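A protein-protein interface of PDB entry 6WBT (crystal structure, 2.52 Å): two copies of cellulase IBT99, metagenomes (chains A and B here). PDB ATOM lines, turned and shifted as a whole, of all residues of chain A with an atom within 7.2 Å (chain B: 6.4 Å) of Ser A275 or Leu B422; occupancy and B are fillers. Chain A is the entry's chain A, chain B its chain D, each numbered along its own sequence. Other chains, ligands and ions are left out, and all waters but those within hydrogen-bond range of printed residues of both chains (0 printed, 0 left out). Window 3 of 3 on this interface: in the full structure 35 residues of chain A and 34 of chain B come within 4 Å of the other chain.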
ATOM      1  N   VAL A 107      -2.648  16.037  -9.230  1.00  0.00           N
ATOM      2  CA  VAL A 107      -2.941  17.467  -9.227  1.00  0.00           C
ATOM      3  C   VAL A 107      -4.235  17.713  -9.990  1.00  0.00           C
ATOM      4  O   VAL A 107      -4.319  17.464 -11.197  1.00  0.00           O
ATOM      5  CB  VAL A 107      -1.782  18.269  -9.832  1.00  0.00           C
ATOM      6  CG1 VAL A 107      -2.187  19.726 -10.020  1.00  0.00           C
ATOM      7  CG2 VAL A 107      -0.550  18.164  -8.953  1.00  0.00           C
ATOM      8  N   HIS A 246      -0.223  32.036  -2.730  1.00  0.00           N
ATOM      9  CA  HIS A 246       0.549  30.799  -2.710  1.00  0.00           C
ATOM     10  C   HIS A 246       1.025  30.418  -4.105  1.00  0.00           C
ATOM     11  O   HIS A 246       2.106  29.837  -4.256  1.00  0.00           O
ATOM     12  CB  HIS A 246      -0.293  29.674  -2.106  1.00  0.00           C
ATOM     13  CG  HIS A 246       0.327  28.317  -2.231  1.00  0.00           C
ATOM     14  ND1 HIS A 246       1.161  27.789  -1.269  1.00  0.00           N
ATOM     15  CD2 HIS A 246       0.230  27.379  -3.202  1.00  0.00           C
ATOM     16  CE1 HIS A 246       1.553  26.583  -1.643  1.00  0.00           C
ATOM     17  NE2 HIS A 246       1.003  26.311  -2.812  1.00  0.00           N
ATOM     18  N   ASN A 250       5.217  30.411  -4.995  1.00  0.00           N
ATOM     19  CA  ASN A 250       5.874  29.142  -5.283  1.00  0.00           C
ATOM     20  C   ASN A 250       6.922  29.257  -6.381  1.00  0.00           C
ATOM     21  O   ASN A 250       7.749  28.350  -6.524  1.00  0.00           O
ATOM     22  CB  ASN A 250       4.840  28.083  -5.674  1.00  0.00           C
ATOM     23  CG  ASN A 250       4.455  27.187  -4.513  1.00  0.00           C
ATOM     24  OD1 ASN A 250       3.476  27.441  -3.817  1.00  0.00           O
ATOM     25  ND2 ASN A 250       5.232  26.131  -4.300  1.00  0.00           N
ATOM     26  N   LEU A 253      11.028  28.841  -5.590  1.00  0.00           N
ATOM     27  CA  LEU A 253      11.782  27.592  -5.643  1.00  0.00           C
ATOM     28  C   LEU A 253      12.164  27.238  -7.074  1.00  0.00           C
ATOM     29  O   LEU A 253      13.292  26.800  -7.330  1.00  0.00           O
ATOM     30  CB  LEU A 253      10.975  26.458  -5.008  1.00  0.00           C
ATOM     31  CG  LEU A 253      10.867  26.402  -3.480  1.00  0.00           C
ATOM     32  CD1 LEU A 253      12.239  26.558  -2.837  1.00  0.00           C
ATOM     33  CD2 LEU A 253       9.884  27.430  -2.931  1.00  0.00           C
ATOM     34  N   MET A 257      16.159  26.933  -8.561  1.00  0.00           N
ATOM     35  CA  MET A 257      16.767  25.683  -9.003  1.00  0.00           C
ATOM     36  C   MET A 257      17.210  25.775 -10.460  1.00  0.00           C
ATOM     37  O   MET A 257      18.267  25.266 -10.830  1.00  0.00           O
ATOM     38  CB  MET A 257      15.789  24.521  -8.817  1.00  0.00           C
ATOM     39  CG  MET A 257      15.320  24.337  -7.382  1.00  0.00           C
ATOM     40  SD  MET A 257      13.871  23.043  -7.196  1.00  0.00           S
ATOM     41  CE  MET A 257      14.851  21.418  -7.633  1.00  0.00           C
ATOM     42  N   GLN A 268       4.152  25.327 -11.422  1.00  0.00           N
ATOM     43  CA  GLN A 268       3.920  24.874 -10.056  1.00  0.00           C
ATOM     44  C   GLN A 268       3.329  23.470 -10.018  1.00  0.00           C
ATOM     45  O   GLN A 268       3.598  22.709  -9.080  1.00  0.00           O
ATOM     46  CB  GLN A 268       2.997  25.867  -9.352  1.00  0.00           C
ATOM     47  CG  GLN A 268       2.655  25.539  -7.918  1.00  0.00           C
ATOM     48  CD  GLN A 268       1.449  26.317  -7.434  1.00  0.00           C
ATOM     49  OE1 GLN A 268       1.294  26.570  -6.239  1.00  0.00           O
ATOM     50  NE2 GLN A 268       0.582  26.699  -8.364  1.00  0.00           N
ATOM     51  N   TYR A 269       2.534  23.104 -11.022  1.00  0.00           N
ATOM     52  CA  TYR A 269       1.849  21.818 -11.026  1.00  0.00           C
ATOM     53  C   TYR A 269       2.620  20.724 -11.754  1.00  0.00           C
ATOM     54  O   TYR A 269       2.400  19.541 -11.470  1.00  0.00           O
ATOM     55  CB  TYR A 269       0.461  21.963 -11.657  1.00  0.00           C
ATOM     56  CG  TYR A 269      -0.325  23.142 -11.128  1.00  0.00           C
ATOM     57  CD1 TYR A 269      -0.539  24.265 -11.915  1.00  0.00           C
ATOM     58  CD2 TYR A 269      -0.840  23.136  -9.839  1.00  0.00           C
ATOM     59  CE1 TYR A 269      -1.252  25.348 -11.435  1.00  0.00           C
ATOM     60  CE2 TYR A 269      -1.554  24.213  -9.350  1.00  0.00           C
ATOM     61  CZ  TYR A 269      -1.758  25.316 -10.152  1.00  0.00           C
ATOM     62  OH  TYR A 269      -2.468  26.391  -9.670  1.00  0.00           O
ATOM     63  N   LEU A 271       6.350  20.763 -12.280  1.00  0.00           N
ATOM     64  CA  LEU A 271       7.608  20.524 -11.587  1.00  0.00           C
ATOM     65  C   LEU A 271       7.413  20.147 -10.126  1.00  0.00           C
ATOM     66  O   LEU A 271       8.303  19.520  -9.539  1.00  0.00           O
ATOM     67  CB  LEU A 271       8.506  21.759 -11.681  1.00  0.00           C
ATOM     68  CG  LEU A 271       8.946  22.159 -13.091  1.00  0.00           C
ATOM     69  CD1 LEU A 271       9.802  23.413 -13.051  1.00  0.00           C
ATOM     70  CD2 LEU A 271       9.692  21.016 -13.763  1.00  0.00           C
ATOM     71  N   MET A 272       6.284  20.513  -9.526  1.00  0.00           N
ATOM     72  CA  MET A 272       6.035  20.199  -8.123  1.00  0.00           C
ATOM     73  C   MET A 272       4.630  19.644  -7.873  1.00  0.00           C
ATOM     74  O   MET A 272       3.835  20.272  -7.176  1.00  0.00           O
ATOM     75  CB  MET A 272       6.250  21.449  -7.261  1.00  0.00           C
ATOM     76  CG  MET A 272       7.600  22.125  -7.460  1.00  0.00           C
ATOM     77  SD  MET A 272       7.647  23.977  -6.844  1.00  0.00           S
ATOM     78  CE  MET A 272       7.810  23.670  -4.926  1.00  0.00           C
ATOM     79  N   PRO A 273       4.317  18.468  -8.434  1.00  0.00           N
ATOM     80  CA  PRO A 273       3.011  17.863  -8.134  1.00  0.00           C
ATOM     81  C   PRO A 273       2.899  17.367  -6.703  1.00  0.00           C
ATOM     82  O   PRO A 273       1.781  17.277  -6.181  1.00  0.00           O
ATOM     83  CB  PRO A 273       2.917  16.711  -9.143  1.00  0.00           C
ATOM     84  CG  PRO A 273       4.330  16.357  -9.425  1.00  0.00           C
ATOM     85  CD  PRO A 273       5.086  17.655  -9.392  1.00  0.00           C
ATOM     86  N   ASP A 274       4.020  17.045  -6.054  1.00  0.00           N
ATOM     87  CA  ASP A 274       3.972  16.606  -4.663  1.00  0.00           C
ATOM     88  C   ASP A 274       3.434  17.707  -3.757  1.00  0.00           C
ATOM     89  O   ASP A 274       2.545  17.471  -2.931  1.00  0.00           O
ATOM     90  CB  ASP A 274       5.362  16.165  -4.200  1.00  0.00           C
ATOM     91  CG  ASP A 274       5.658  14.718  -4.534  1.00  0.00           C
ATOM     92  OD1 ASP A 274       4.739  14.012  -5.003  1.00  0.00           O
ATOM     93  OD2 ASP A 274       6.809  14.283  -4.324  1.00  0.00           O
ATOM     94  N   SER A 275       3.961  18.925  -3.904  1.00  0.00           N
ATOM     95  CA  SER A 275       3.563  20.023  -3.032  1.00  0.00           C
ATOM     96  C   SER A 275       2.183  20.577  -3.358  1.00  0.00           C
ATOM     97  O   SER A 275       1.697  21.444  -2.624  1.00  0.00           O
ATOM     98  CB  SER A 275       4.597  21.147  -3.104  1.00  0.00           C
ATOM     99  OG  SER A 275       4.678  21.680  -4.414  1.00  0.00           O
ATOM    100  N   ILE A 276       1.543  20.106  -4.423  1.00  0.00           N
ATOM    101  CA  ILE A 276       0.225  20.587  -4.813  1.00  0.00           C
ATOM    102  C   ILE A 276      -0.877  19.634  -4.369  1.00  0.00           C
ATOM    103  O   ILE A 276      -1.936  20.075  -3.922  1.00  0.00           O
ATOM    104  CB  ILE A 276       0.176  20.831  -6.338  1.00  0.00           C
ATOM    105  CG1 ILE A 276       1.122  21.971  -6.710  1.00  0.00           C
ATOM    106  CG2 ILE A 276      -1.236  21.156  -6.786  1.00  0.00           C
ATOM    107  CD1 ILE A 276       0.898  23.221  -5.889  1.00  0.00           C
ATOM    108  N   VAL A 277      -0.643  18.323  -4.482  1.00  0.00           N
ATOM    109  CA  VAL A 277      -1.617  17.353  -3.991  1.00  0.00           C
ATOM    110  C   VAL A 277      -1.816  17.510  -2.489  1.00  0.00           C
ATOM    111  O   VAL A 277      -2.924  17.312  -1.974  1.00  0.00           O
ATOM    112  CB  VAL A 277      -1.179  15.922  -4.362  1.00  0.00           C
ATOM    113  CG1 VAL A 277      -2.177  14.899  -3.840  1.00  0.00           C
ATOM    114  CG2 VAL A 277      -1.026  15.790  -5.870  1.00  0.00           C
ATOM    115  N   ASP A 278      -0.759  17.883  -1.765  1.00  0.00           N
ATOM    116  CA  ASP A 278      -0.880  18.125  -0.332  1.00  0.00           C
ATOM    117  C   ASP A 278      -1.541  19.463  -0.029  1.00  0.00           C
ATOM    118  O   ASP A 278      -2.215  19.598   0.999  1.00  0.00           O
ATOM    119  CB  ASP A 278       0.499  18.065   0.329  1.00  0.00           C
ATOM    120  CG  ASP A 278       1.113  16.679   0.274  1.00  0.00           C
ATOM    121  OD1 ASP A 278       1.236  16.125  -0.838  1.00  0.00           O
ATOM    122  OD2 ASP A 278       1.476  16.148   1.343  1.00  0.00           O
ATOM    123  N   TYR A 279      -1.365  20.457  -0.903  1.00  0.00           N
ATOM    124  CA  TYR A 279      -1.907  21.787  -0.645  1.00  0.00           C
ATOM    125  C   TYR A 279      -3.402  21.869  -0.927  1.00  0.00           C
ATOM    126  O   TYR A 279      -4.107  22.647  -0.273  1.00  0.00           O
ATOM    127  CB  TYR A 279      -1.154  22.826  -1.480  1.00  0.00           C
ATOM    128  CG  TYR A 279      -1.820  24.184  -1.534  1.00  0.00           C
ATOM    129  CD1 TYR A 279      -1.789  25.039  -0.440  1.00  0.00           C
ATOM    130  CD2 TYR A 279      -2.469  24.615  -2.684  1.00  0.00           C
ATOM    131  CE1 TYR A 279      -2.395  26.283  -0.486  1.00  0.00           C
ATOM    132  CE2 TYR A 279      -3.077  25.855  -2.740  1.00  0.00           C
ATOM    133  CZ  TYR A 279      -3.036  26.684  -1.639  1.00  0.00           C
ATOM    134  OH  TYR A 279      -3.639  27.920  -1.692  1.00  0.00           O
ATOM    135  N   MET A 280      -3.902  21.088  -1.876  1.00  0.00           N
ATOM    136  CA  MET A 280      -5.305  21.166  -2.269  1.00  0.00           C
ATOM    137  C   MET A 280      -6.218  20.373  -1.340  1.00  0.00           C
ATOM    138  O   MET A 280      -5.797  19.401  -0.713  1.00  0.00           O
ATOM    139  CB  MET A 280      -5.480  20.678  -3.708  1.00  0.00           C
ATOM    140  CG  MET A 280      -4.896  21.614  -4.751  1.00  0.00           C
ATOM    141  SD  MET A 280      -5.156  20.973  -6.573  1.00  0.00           S
ATOM    142  CE  MET A 280      -4.557  22.559  -7.537  1.00  0.00           C
ATOM    143  N   THR B 413      15.292  15.911 -12.773  1.00  0.00           N
ATOM    144  CA  THR B 413      13.898  16.330 -12.885  1.00  0.00           C
ATOM    145  C   THR B 413      13.234  15.749 -14.128  1.00  0.00           C
ATOM    146  O   THR B 413      12.030  15.472 -14.115  1.00  0.00           O
ATOM    147  CB  THR B 413      13.810  17.857 -12.901  1.00  0.00           C
ATOM    148  OG1 THR B 413      14.544  18.393 -11.792  1.00  0.00           O
ATOM    149  CG2 THR B 413      12.361  18.315 -12.802  1.00  0.00           C
ATOM    150  N   SER B 420       8.808  14.660  -8.691  1.00  0.00           N
ATOM    151  CA  SER B 420       8.854  16.112  -8.790  1.00  0.00           C
ATOM    152  C   SER B 420      10.302  16.577  -8.735  1.00  0.00           C
ATOM    153  O   SER B 420      11.223  15.792  -8.492  1.00  0.00           O
ATOM    154  CB  SER B 420       8.036  16.772  -7.674  1.00  0.00           C
ATOM    155  OG  SER B 420       8.520  16.392  -6.397  1.00  0.00           O
ATOM    156  N   SER B 421      10.493  17.879  -8.964  1.00  0.00           N
ATOM    157  CA  SER B 421      11.824  18.464  -8.844  1.00  0.00           C
ATOM    158  C   SER B 421      12.271  18.534  -7.390  1.00  0.00           C
ATOM    159  O   SER B 421      13.477  18.524  -7.114  1.00  0.00           O
ATOM    160  CB  SER B 421      11.847  19.856  -9.474  1.00  0.00           C
ATOM    161  OG  SER B 421      10.998  20.748  -8.773  1.00  0.00           O
ATOM    162  N   LEU B 422      11.322  18.605  -6.454  1.00  0.00           N
ATOM    163  CA  LEU B 422      11.673  18.619  -5.037  1.00  0.00           C
ATOM    164  C   LEU B 422      12.371  17.326  -4.636  1.00  0.00           C
ATOM    165  O   LEU B 422      13.424  17.348  -3.986  1.00  0.00           O
ATOM    166  CB  LEU B 422      10.419  18.840  -4.190  1.00  0.00           C
ATOM    167  CG  LEU B 422       9.682  20.163  -4.397  1.00  0.00           C
ATOM    168  CD1 LEU B 422       8.387  20.186  -3.597  1.00  0.00           C
ATOM    169  CD2 LEU B 422      10.572  21.334  -4.013  1.00  0.00           C
ATOM    170  N   VAL B 423      11.796  16.183  -5.018  1.00  0.00           N
ATOM    171  CA  VAL B 423      12.435  14.903  -4.742  1.00  0.00           C
ATOM    172  C   VAL B 423      13.730  14.771  -5.533  1.00  0.00           C
ATOM    173  O   VAL B 423      14.684  14.133  -5.073  1.00  0.00           O
ATOM    174  CB  VAL B 423      11.461  13.748  -5.046  1.00  0.00           C
ATOM    175  CG1 VAL B 423      12.103  12.402  -4.740  1.00  0.00           C
ATOM    176  CG2 VAL B 423      10.175  13.920  -4.251  1.00  0.00           C
ATOM    177  N   ALA B 424      13.794  15.382  -6.719  1.00  0.00           N
ATOM    178  CA  ALA B 424      14.996  15.287  -7.542  1.00  0.00           C
ATOM    179  C   ALA B 424      16.192  15.939  -6.859  1.00  0.00           C
ATOM    180  O   ALA B 424      17.311  15.414  -6.920  1.00  0.00           O
ATOM    181  CB  ALA B 424      14.746  15.925  -8.908  1.00  0.00           C
ATOM    182  N   LYS B 425      15.980  17.084  -6.206  1.00  0.00           N
ATOM    183  CA  LYS B 425      17.083  17.750  -5.521  1.00  0.00           C
ATOM    184  C   LYS B 425      17.533  16.957  -4.301  1.00  0.00           C
ATOM    185  O   LYS B 425      18.736  16.803  -4.061  1.00  0.00           O
ATOM    186  CB  LYS B 425      16.679  19.169  -5.124  1.00  0.00           C
ATOM    187  CG  LYS B 425      17.825  20.004  -4.575  1.00  0.00           C
ATOM    188  CD  LYS B 425      17.362  21.403  -4.206  1.00  0.00           C
ATOM    189  CE  LYS B 425      18.532  22.277  -3.783  1.00  0.00           C
ATOM    190  NZ  LYS B 425      19.515  22.459  -4.886  1.00  0.00           N
ATOM    191  N   LYS B 426      16.579  16.445  -3.517  1.00  0.00           N
ATOM    192  CA  LYS B 426      16.927  15.590  -2.388  1.00  0.00           C
ATOM    193  C   LYS B 426      17.568  14.290  -2.852  1.00  0.00           C
ATOM    194  O   LYS B 426      18.384  13.707  -2.128  1.00  0.00           O
ATOM    195  CB  LYS B 426      15.683  15.298  -1.549  1.00  0.00           C
ATOM    196  CG  LYS B 426      14.999  16.539  -1.000  1.00  0.00           C
ATOM    197  CD  LYS B 426      13.640  16.204  -0.407  1.00  0.00           C
ATOM    198  CE  LYS B 426      13.755  15.185   0.715  1.00  0.00           C
ATOM    199  NZ  LYS B 426      12.425  14.850   1.292  1.00  0.00           N
ATOM    200  N   LEU B 427      17.215  13.823  -4.049  1.00  0.00           N
ATOM    201  CA  LEU B 427      17.804  12.600  -4.581  1.00  0.00           C
ATOM    202  C   LEU B 427      19.216  12.845  -5.100  1.00  0.00           C
ATOM    203  O   LEU B 427      20.113  12.025  -4.876  1.00  0.00           O
ATOM    204  CB  LEU B 427      16.912  12.035  -5.687  1.00  0.00           C
ATOM    205  CG  LEU B 427      16.907  10.526  -5.927  1.00  0.00           C
ATOM    206  CD1 LEU B 427      16.962   9.776  -4.613  1.00  0.00           C
ATOM    207  CD2 LEU B 427      15.654  10.147  -6.693  1.00  0.00           C
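Of the 17 printed residues of chain A, 6 touch a printed residue of chain B. Among the printed residues, 12 pairs touch across the chains.
The backbone NH (N) of Ser B421 sits at hydrogen-bond distance from the backbone carbonyl oxygen (O) of Leu A271 (2.8 Å). The side-chain carboxylate (OD2) of Asp A274 sits at hydrogen-bond distance from the side-chain hydroxyl (OG) of Ser B420, at 3.4 Å.
O of Met A272 lies within hydrogen-bond range of OG of Ser A275, at 3.2 Å.
Among the printed residues, pairs that only touch across the chains: Met A257 with Ser B421, Leu A271 with Ser B420, Asp A274 with Val B423, Pro A273 with Ser B420, Met A272 with Leu B422, Met A257 with Lys B425, Met A272 with Ser B421, Leu A271 with Thr B413, Ser A275 with Leu B422 and Met A272 with Ser B420.
Ser A275 touches just one residue of chain B: Leu B422 (3.9 Å). Printed residues of chain A within 4 Å of Leu B422: Met A272 (3.7 Å) and Ser A275 (3.9 Å). Of the printed residues of chain A, Ser B421 touches Met A257 (3.2 Å), Leu A271 (2.8 Å) and Met A272 (3.9 Å). Of the printed residues of chain B, Met A272 touches Ser B420 (3.99 Å), Ser B421 (3.9 Å) and Leu B422 (3.7 Å). Of the printed residues of chain B, Asp A274 touches Ser B420 (3.4 Å) and Val B423 (3.4 Å). Gln A268 touches none of the printed residues of chain B. The nearest residue of chain B that does not touch Ser A275 is Ser B420 (5.8 Å). The nearest residue of chain A that does not touch Leu B422 is Leu A271 (4.4 Å). The nearest printed residue of chain B that does not touch Met A272 is Thr B413 (7.2 Å).
No position is printed for both chains. Of the 12 pairs that touch across the chains among the printed residues, none has its exchanged pair printed and touching as well.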
